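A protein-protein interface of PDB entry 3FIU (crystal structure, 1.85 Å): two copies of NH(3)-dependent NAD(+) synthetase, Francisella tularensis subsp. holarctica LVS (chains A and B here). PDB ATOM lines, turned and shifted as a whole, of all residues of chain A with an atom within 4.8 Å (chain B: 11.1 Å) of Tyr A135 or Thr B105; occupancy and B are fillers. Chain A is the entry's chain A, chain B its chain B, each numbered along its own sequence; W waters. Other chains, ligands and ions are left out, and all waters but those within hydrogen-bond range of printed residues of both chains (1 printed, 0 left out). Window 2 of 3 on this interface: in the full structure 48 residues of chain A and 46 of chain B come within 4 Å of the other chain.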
ATOM      1  N   GLU A  30      12.738  -6.637   7.171  1.00  0.00           N
ATOM      2  CA  GLU A  30      11.418  -6.062   7.425  1.00  0.00           C
ATOM      3  C   GLU A  30      11.067  -6.031   8.937  1.00  0.00           C
ATOM      4  O   GLU A  30      10.226  -5.232   9.382  1.00  0.00           O
ATOM      5  CB  GLU A  30      10.359  -6.806   6.596  1.00  0.00           C
ATOM      6  CG  GLU A  30      10.494  -6.561   5.079  1.00  0.00           C
ATOM      7  CD  GLU A  30       9.715  -7.564   4.224  1.00  0.00           C
ATOM      8  OE1 GLU A  30       8.635  -8.050   4.655  1.00  0.00           O
ATOM      9  OE2 GLU A  30      10.191  -7.861   3.105  1.00  0.00           O
ATOM     10  N   TYR A 131      12.285 -19.373   9.671  1.00  0.00           N
ATOM     11  CA  TYR A 131      11.260 -18.312   9.656  1.00  0.00           C
ATOM     12  C   TYR A 131      11.820 -17.006   9.085  1.00  0.00           C
ATOM     13  O   TYR A 131      11.232 -16.394   8.188  1.00  0.00           O
ATOM     14  CB  TYR A 131      10.700 -18.046  11.067  1.00  0.00           C
ATOM     15  CG  TYR A 131       9.543 -17.062  11.024  1.00  0.00           C
ATOM     16  CD1 TYR A 131       8.235 -17.508  10.869  1.00  0.00           C
ATOM     17  CD2 TYR A 131       9.772 -15.686  11.083  1.00  0.00           C
ATOM     18  CE1 TYR A 131       7.170 -16.604  10.797  1.00  0.00           C
ATOM     19  CE2 TYR A 131       8.716 -14.773  11.009  1.00  0.00           C
ATOM     20  CZ  TYR A 131       7.414 -15.247  10.848  1.00  0.00           C
ATOM     21  OH  TYR A 131       6.353 -14.353  10.780  1.00  0.00           O
ATOM     22  N   ALA A 132      12.960 -16.582   9.613  1.00  0.00           N
ATOM     23  CA  ALA A 132      13.574 -15.315   9.249  1.00  0.00           C
ATOM     24  C   ALA A 132      13.805 -15.226   7.729  1.00  0.00           C
ATOM     25  O   ALA A 132      13.528 -14.179   7.090  1.00  0.00           O
ATOM     26  CB  ALA A 132      14.908 -15.160   9.991  1.00  0.00           C
ATOM     27  N   GLN A 133      14.315 -16.307   7.150  1.00  0.00           N
ATOM     28  CA  GLN A 133      14.621 -16.276   5.720  1.00  0.00           C
ATOM     29  C   GLN A 133      13.348 -16.268   4.901  1.00  0.00           C
ATOM     30  O   GLN A 133      13.292 -15.601   3.860  1.00  0.00           O
ATOM     31  CB  GLN A 133      15.556 -17.415   5.298  1.00  0.00           C
ATOM     32  CG  GLN A 133      16.044 -17.246   3.837  1.00  0.00           C
ATOM     33  CD  GLN A 133      17.104 -18.249   3.423  1.00  0.00           C
ATOM     34  OE1 GLN A 133      17.429 -19.208   4.157  1.00  0.00           O
ATOM     35  NE2 GLN A 133      17.665 -18.028   2.234  1.00  0.00           N
ATOM     36  N   GLN A 134      12.322 -16.986   5.367  1.00  0.00           N
ATOM     37  CA  GLN A 134      11.042 -16.997   4.657  1.00  0.00           C
ATOM     38  C   GLN A 134      10.324 -15.633   4.693  1.00  0.00           C
ATOM     39  O   GLN A 134       9.641 -15.287   3.735  1.00  0.00           O
ATOM     40  CB  GLN A 134      10.123 -18.098   5.184  1.00  0.00           C
ATOM     41  CG  GLN A 134       8.810 -18.169   4.427  1.00  0.00           C
ATOM     42  CD  GLN A 134       8.076 -19.480   4.605  1.00  0.00           C
ATOM     43  OE1 GLN A 134       8.651 -20.475   5.059  1.00  0.00           O
ATOM     44  NE2 GLN A 134       6.784 -19.491   4.237  1.00  0.00           N
ATOM     45  N   TYR A 135      10.489 -14.868   5.772  1.00  0.00           N
ATOM     46  CA  TYR A 135       9.727 -13.615   5.973  1.00  0.00           C
ATOM     47  C   TYR A 135      10.588 -12.362   6.038  1.00  0.00           C
ATOM     48  O   TYR A 135      10.117 -11.317   6.502  1.00  0.00           O
ATOM     49  CB  TYR A 135       8.821 -13.702   7.219  1.00  0.00           C
ATOM     50  CG  TYR A 135       7.703 -14.702   7.052  1.00  0.00           C
ATOM     51  CD1 TYR A 135       6.470 -14.315   6.519  1.00  0.00           C
ATOM     52  CD2 TYR A 135       7.884 -16.039   7.401  1.00  0.00           C
ATOM     53  CE1 TYR A 135       5.442 -15.237   6.350  1.00  0.00           C
ATOM     54  CE2 TYR A 135       6.864 -16.977   7.235  1.00  0.00           C
ATOM     55  CZ  TYR A 135       5.642 -16.560   6.708  1.00  0.00           C
ATOM     56  OH  TYR A 135       4.636 -17.471   6.526  1.00  0.00           O
ATOM     57  N   ASN A 136      11.835 -12.468   5.572  1.00  0.00           N
ATOM     58  CA  ASN A 136      12.828 -11.360   5.625  1.00  0.00           C
ATOM     59  C   ASN A 136      12.934 -10.686   6.999  1.00  0.00           C
ATOM     60  O   ASN A 136      12.790  -9.469   7.121  1.00  0.00           O
ATOM     61  CB  ASN A 136      12.583 -10.298   4.522  1.00  0.00           C
ATOM     62  CG  ASN A 136      13.743  -9.301   4.376  1.00  0.00           C
ATOM     63  OD1 ASN A 136      13.522  -8.113   4.115  1.00  0.00           O
ATOM     64  ND2 ASN A 136      14.973  -9.775   4.553  1.00  0.00           N
ATOM     65  N   ARG A 137      13.168 -11.485   8.034  1.00  0.00           N
ATOM     66  CA  ARG A 137      13.353 -10.954   9.382  1.00  0.00           C
ATOM     67  C   ARG A 137      14.785 -11.113   9.820  1.00  0.00           C
ATOM     68  O   ARG A 137      15.519 -11.900   9.232  1.00  0.00           O
ATOM     69  CB  ARG A 137      12.476 -11.715  10.398  1.00  0.00           C
ATOM     70  CG  ARG A 137      10.967 -11.728  10.053  1.00  0.00           C
ATOM     71  CD  ARG A 137      10.318 -10.332  10.073  1.00  0.00           C
ATOM     72  NE  ARG A 137       8.902 -10.432   9.701  1.00  0.00           N
ATOM     73  CZ  ARG A 137       7.922 -10.751  10.545  1.00  0.00           C
ATOM     74  NH1 ARG A 137       8.183 -10.956  11.845  1.00  0.00           N
ATOM     75  NH2 ARG A 137       6.666 -10.841  10.101  1.00  0.00           N
ATOM     76  N   TYR B  94      15.997 -34.008   8.649  1.00  0.00           N
ATOM     77  CA  TYR B  94      15.539 -32.902   7.811  1.00  0.00           C
ATOM     78  C   TYR B  94      14.031 -33.006   7.580  1.00  0.00           C
ATOM     79  O   TYR B  94      13.306 -32.023   7.732  1.00  0.00           O
ATOM     80  CB  TYR B  94      16.275 -32.838   6.460  1.00  0.00           C
ATOM     81  CG  TYR B  94      15.621 -31.807   5.560  1.00  0.00           C
ATOM     82  CD1 TYR B  94      14.767 -32.197   4.513  1.00  0.00           C
ATOM     83  CD2 TYR B  94      15.761 -30.457   5.830  1.00  0.00           C
ATOM     84  CE1 TYR B  94      14.130 -31.245   3.727  1.00  0.00           C
ATOM     85  CE2 TYR B  94      15.112 -29.498   5.058  1.00  0.00           C
ATOM     86  CZ  TYR B  94      14.305 -29.901   4.009  1.00  0.00           C
ATOM     87  OH  TYR B  94      13.662 -28.938   3.258  1.00  0.00           O
ATOM     88  N   GLU B  95      13.557 -34.193   7.207  1.00  0.00           N
ATOM     89  CA  GLU B  95      12.125 -34.334   6.905  1.00  0.00           C
ATOM     90  C   GLU B  95      11.244 -33.983   8.116  1.00  0.00           C
ATOM     91  O   GLU B  95      10.244 -33.286   7.962  1.00  0.00           O
ATOM     92  CB  GLU B  95      11.787 -35.716   6.338  1.00  0.00           C
ATOM     93  CG  GLU B  95      12.222 -35.848   4.884  1.00  0.00           C
ATOM     94  CD  GLU B  95      11.967 -37.216   4.311  1.00  0.00           C
ATOM     95  OE1 GLU B  95      11.174 -37.985   4.906  1.00  0.00           O
ATOM     96  OE2 GLU B  95      12.576 -37.520   3.262  1.00  0.00           O
ATOM     97  N   ALA B  96      11.630 -34.459   9.300  1.00  0.00           N
ATOM     98  CA  ALA B  96      10.891 -34.101  10.546  1.00  0.00           C
ATOM     99  C   ALA B  96      10.911 -32.593  10.827  1.00  0.00           C
ATOM    100  O   ALA B  96       9.881 -31.988  11.178  1.00  0.00           O
ATOM    101  CB  ALA B  96      11.454 -34.876  11.710  1.00  0.00           C
ATOM    102  N   PHE B  97      12.094 -31.975  10.711  1.00  0.00           N
ATOM    103  CA  PHE B  97      12.211 -30.527  10.852  1.00  0.00           C
ATOM    104  C   PHE B  97      11.280 -29.793   9.860  1.00  0.00           C
ATOM    105  O   PHE B  97      10.441 -28.966  10.244  1.00  0.00           O
ATOM    106  CB  PHE B  97      13.671 -30.073  10.619  1.00  0.00           C
ATOM    107  CG  PHE B  97      13.829 -28.590  10.642  1.00  0.00           C
ATOM    108  CD1 PHE B  97      13.788 -27.889  11.859  1.00  0.00           C
ATOM    109  CD2 PHE B  97      13.992 -27.872   9.452  1.00  0.00           C
ATOM    110  CE1 PHE B  97      13.899 -26.463  11.881  1.00  0.00           C
ATOM    111  CE2 PHE B  97      14.105 -26.486   9.461  1.00  0.00           C
ATOM    112  CZ  PHE B  97      14.062 -25.771  10.695  1.00  0.00           C
ATOM    113  N   LEU B  98      11.411 -30.132   8.582  1.00  0.00           N
ATOM    114  CA  LEU B  98      10.596 -29.488   7.547  1.00  0.00           C
ATOM    115  C   LEU B  98       9.104 -29.614   7.857  1.00  0.00           C
ATOM    116  O   LEU B  98       8.386 -28.640   7.788  1.00  0.00           O
ATOM    117  CB  LEU B  98      10.889 -30.091   6.156  1.00  0.00           C
ATOM    118  CG  LEU B  98       9.965 -29.610   5.017  1.00  0.00           C
ATOM    119  CD1 LEU B  98      10.201 -28.136   4.724  1.00  0.00           C
ATOM    120  CD2 LEU B  98      10.192 -30.456   3.752  1.00  0.00           C
ATOM    121  N   ALA B  99       8.646 -30.820   8.197  1.00  0.00           N
ATOM    122  CA  ALA B  99       7.228 -31.057   8.450  1.00  0.00           C
ATOM    123  C   ALA B  99       6.762 -30.144   9.573  1.00  0.00           C
ATOM    124  O   ALA B  99       5.693 -29.542   9.488  1.00  0.00           O
ATOM    125  CB  ALA B  99       6.987 -32.530   8.839  1.00  0.00           C
ATOM    126  N   SER B 100       7.602 -30.009  10.603  1.00  0.00           N
ATOM    127  CA  SER B 100       7.236 -29.256  11.809  1.00  0.00           C
ATOM    128  C   SER B 100       7.147 -27.753  11.529  1.00  0.00           C
ATOM    129  O   SER B 100       6.622 -27.001  12.375  1.00  0.00           O
ATOM    130  CB  SER B 100       8.203 -29.539  12.972  1.00  0.00           C
ATOM    131  OG  SER B 100       9.511 -29.033  12.701  1.00  0.00           O
ATOM    132  N   THR B 101       7.603 -27.318  10.344  1.00  0.00           N
ATOM    133  CA  THR B 101       7.557 -25.877  10.000  1.00  0.00           C
ATOM    134  C   THR B 101       6.317 -25.470   9.224  1.00  0.00           C
ATOM    135  O   THR B 101       6.191 -24.320   8.819  1.00  0.00           O
ATOM    136  CB  THR B 101       8.762 -25.387   9.194  1.00  0.00           C
ATOM    137  OG1 THR B 101       8.735 -26.030   7.923  1.00  0.00           O
ATOM    138  CG2 THR B 101      10.130 -25.700   9.930  1.00  0.00           C
ATOM    139  N   GLN B 102       5.383 -26.397   9.073  1.00  0.00           N
ATOM    140  CA  GLN B 102       4.227 -26.197   8.187  1.00  0.00           C
ATOM    141  C   GLN B 102       3.329 -25.014   8.571  1.00  0.00           C
ATOM    142  O   GLN B 102       2.844 -24.297   7.704  1.00  0.00           O
ATOM    143  CB  GLN B 102       3.432 -27.499   8.098  1.00  0.00           C
ATOM    144  CG  GLN B 102       2.800 -27.948   9.396  1.00  0.00           C
ATOM    145  CD  GLN B 102       1.560 -27.169   9.755  1.00  0.00           C
ATOM    146  OE1 GLN B 102       0.800 -26.736   8.881  1.00  0.00           O
ATOM    147  NE2 GLN B 102       1.345 -26.983  11.045  1.00  0.00           N
ATOM    148  N   SER B 103       3.161 -24.761   9.869  1.00  0.00           N
ATOM    149  CA  SER B 103       2.289 -23.668  10.307  1.00  0.00           C
ATOM    150  C   SER B 103       2.726 -22.304   9.809  1.00  0.00           C
ATOM    151  O   SER B 103       1.891 -21.389   9.707  1.00  0.00           O
ATOM    152  CB  SER B 103       2.170 -23.640  11.836  1.00  0.00           C
ATOM    153  OG  SER B 103       3.424 -23.344  12.456  1.00  0.00           O
ATOM    154  N   PHE B 104       4.016 -22.155   9.493  1.00  0.00           N
ATOM    155  CA  PHE B 104       4.515 -20.850   9.033  1.00  0.00           C
ATOM    156  C   PHE B 104       5.059 -20.787   7.600  1.00  0.00           C
ATOM    157  O   PHE B 104       5.509 -19.737   7.159  1.00  0.00           O
ATOM    158  CB  PHE B 104       5.457 -20.148  10.067  1.00  0.00           C
ATOM    159  CG  PHE B 104       6.804 -20.814  10.283  1.00  0.00           C
ATOM    160  CD1 PHE B 104       7.128 -21.368  11.529  1.00  0.00           C
ATOM    161  CD2 PHE B 104       7.786 -20.807   9.277  1.00  0.00           C
ATOM    162  CE1 PHE B 104       8.409 -21.966  11.768  1.00  0.00           C
ATOM    163  CE2 PHE B 104       9.045 -21.401   9.491  1.00  0.00           C
ATOM    164  CZ  PHE B 104       9.359 -21.983  10.726  1.00  0.00           C
ATOM    165  N   THR B 105       5.015 -21.917   6.889  1.00  0.00           N
ATOM    166  CA  THR B 105       5.392 -21.970   5.469  1.00  0.00           C
ATOM    167  C   THR B 105       4.160 -21.678   4.622  1.00  0.00           C
ATOM    168  O   THR B 105       3.673 -20.540   4.604  1.00  0.00           O
ATOM    169  CB  THR B 105       5.995 -23.333   5.056  1.00  0.00           C
ATOM    170  OG1 THR B 105       7.088 -23.660   5.923  1.00  0.00           O
ATOM    171  CG2 THR B 105       6.527 -23.263   3.618  1.00  0.00           C
ATOM    172  N   GLN B 112      10.964 -23.468  -0.578  1.00  0.00           N
ATOM    173  CA  GLN B 112      12.153 -22.747  -1.014  1.00  0.00           C
ATOM    174  C   GLN B 112      13.382 -23.624  -0.991  1.00  0.00           C
ATOM    175  O   GLN B 112      13.714 -24.240   0.033  1.00  0.00           O
ATOM    176  CB  GLN B 112      12.413 -21.505  -0.159  1.00  0.00           C
ATOM    177  CG  GLN B 112      13.702 -20.760  -0.527  1.00  0.00           C
ATOM    178  CD  GLN B 112      13.689 -20.266  -1.973  1.00  0.00           C
ATOM    179  OE1 GLN B 112      12.703 -19.667  -2.427  1.00  0.00           O
ATOM    180  NE2 GLN B 112      14.781 -20.514  -2.705  1.00  0.00           N
ATOM    181  N   LEU B 113      14.074 -23.636  -2.125  1.00  0.00           N
ATOM    182  CA  LEU B 113      15.275 -24.427  -2.288  1.00  0.00           C
ATOM    183  C   LEU B 113      16.420 -23.908  -1.423  1.00  0.00           C
ATOM    184  O   LEU B 113      17.154 -24.715  -0.835  1.00  0.00           O
ATOM    185  CB  LEU B 113      15.687 -24.459  -3.756  1.00  0.00           C
ATOM    186  CG  LEU B 113      16.443 -25.681  -4.259  1.00  0.00           C
ATOM    187  CD1 LEU B 113      15.941 -26.970  -3.621  1.00  0.00           C
ATOM    188  CD2 LEU B 113      16.297 -25.731  -5.785  1.00  0.00           C
ATOM    189  N   ILE B 115      16.093 -22.159   1.386  1.00  0.00           N
ATOM    190  CA  ILE B 115      15.706 -22.469   2.768  1.00  0.00           C
ATOM    191  C   ILE B 115      16.076 -23.922   3.117  1.00  0.00           C
ATOM    192  O   ILE B 115      16.690 -24.174   4.158  1.00  0.00           O
ATOM    193  CB  ILE B 115      14.212 -22.127   3.041  1.00  0.00           C
ATOM    194  CG1 ILE B 115      14.071 -20.601   3.203  1.00  0.00           C
ATOM    195  CG2 ILE B 115      13.691 -22.867   4.277  1.00  0.00           C
ATOM    196  CD1 ILE B 115      12.651 -20.029   2.982  1.00  0.00           C
ATOM    197  N   LYS B 116      15.730 -24.852   2.224  1.00  0.00           N
ATOM    198  CA  LYS B 116      16.169 -26.235   2.325  1.00  0.00           C
ATOM    199  C   LYS B 116      17.695 -26.382   2.447  1.00  0.00           C
ATOM    200  O   LYS B 116      18.187 -27.092   3.335  1.00  0.00           O
ATOM    201  CB  LYS B 116      15.691 -27.015   1.094  1.00  0.00           C
ATOM    202  CG  LYS B 116      16.047 -28.490   1.120  1.00  0.00           C
ATOM    203  CD  LYS B 116      15.429 -29.156  -0.114  1.00  0.00           C
ATOM    204  CE  LYS B 116      15.929 -30.558  -0.376  1.00  0.00           C
ATOM    205  NZ  LYS B 116      15.537 -30.919  -1.775  1.00  0.00           N
ATOM    206  N   ASN B 118      19.905 -24.357   3.387  1.00  0.00           N
ATOM    207  CA  ASN B 118      20.421 -23.790   4.650  1.00  0.00           C
ATOM    208  C   ASN B 118      20.086 -24.674   5.864  1.00  0.00           C
ATOM    209  O   ASN B 118      20.926 -24.843   6.760  1.00  0.00           O
ATOM    210  CB  ASN B 118      19.947 -22.332   4.861  1.00  0.00           C
ATOM    211  CG  ASN B 118      20.588 -21.347   3.870  1.00  0.00           C
ATOM    212  OD1 ASN B 118      21.671 -21.589   3.349  1.00  0.00           O
ATOM    213  ND2 ASN B 118      19.925 -20.216   3.642  1.00  0.00           N
ATOM    214  N   ALA B 119      18.876 -25.233   5.890  1.00  0.00           N
ATOM    215  CA  ALA B 119      18.476 -26.168   6.962  1.00  0.00           C
ATOM    216  C   ALA B 119      19.399 -27.370   6.983  1.00  0.00           C
ATOM    217  O   ALA B 119      19.862 -27.812   8.026  1.00  0.00           O
ATOM    218  CB  ALA B 119      17.010 -26.633   6.757  1.00  0.00           C
HETATM  219  O   HOH W   1      21.053 -17.888   1.913  1.00  0.00           O
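O of Thr B105 sits close to NE2 of Gln A134 (3.3 Å). The backbone carbonyl oxygen (O) of Phe B104 is in hydrogen-bond range of the side-chain amide nitrogen (NE2) of Gln A134, 3.2 Å away. The side-chain amide oxygen (OE1) of Gln A133 sits at hydrogen-bond distance from the side-chain amide nitrogen (ND2) of Asn B118, at 2.7 Å. OH of Tyr A135 lies within hydrogen-bond range of O of Phe B104 (2.5 Å).
The backbone carbonyl oxygen (O) of Thr B101 sits at hydrogen-bond distance from the side-chain hydroxyl (OG1) of Thr B105.
Tyr A131 touches Phe B104 (CD1 to CG, 3.6 Å). Ile B115 touches Gln A133 (CG1 to OE1, 3.8 Å). CA of Gln A134 touches CD1 of Ile B115 (3.8 Å). OH of Tyr A135 touches O of Thr B105 (3.7 Å).
Thr B105 touches just these residues of chain A: Gln A134 (3.1 Å) and Tyr A135 (3.7 Å). Printed residues of chain B within 4 Å of Tyr A131: Phe B104. Ala A132 touches none of the printed residues of chain B. Of chain B, only Phe B104, Thr B105 and Ile B115 come within 4 Å of Gln A134. No residue of chain B comes within 4 Å of Arg A137. Printed residues of chain A within 4 Å of Ile B115: Gln A133 and Gln A134. Printed residues of chain A within 4 Å of Asn B118: Gln A133 (2.7 Å). Printed residues of chain B within 4 Å of Gln A133: Ile B115 and Asn B118. Printed residues of chain A within 4 Å of Phe B104: Tyr A131 (3.6 Å), Gln A134 (3.2 Å) and Tyr A135 (2.5 Å). The nearest residue of chain B that does not touch Tyr A135 is Ser B103 (5.7 Å). The nearest printed residue of chain A that does not touch Thr B105 is Tyr A131 (6.8 Å). The nearest printed residue of chain B that does not touch Gln A133 is Gln B112 (5.5 Å).
Of the 8 printed residues of chain A, 4 touch a printed residue of chain B. Among the printed residues, 8 pairs touch across the chains.
No position is printed for both chains. Of the 8 pairs that touch across the chains among the printed residues, none has its exchanged pair printed and touching as well.
Water W1 bridges the side-chain amide nitrogen of Asn B118 (3.1 Å) and the side-chain amide nitrogen of Gln A133 (3.4 Å).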
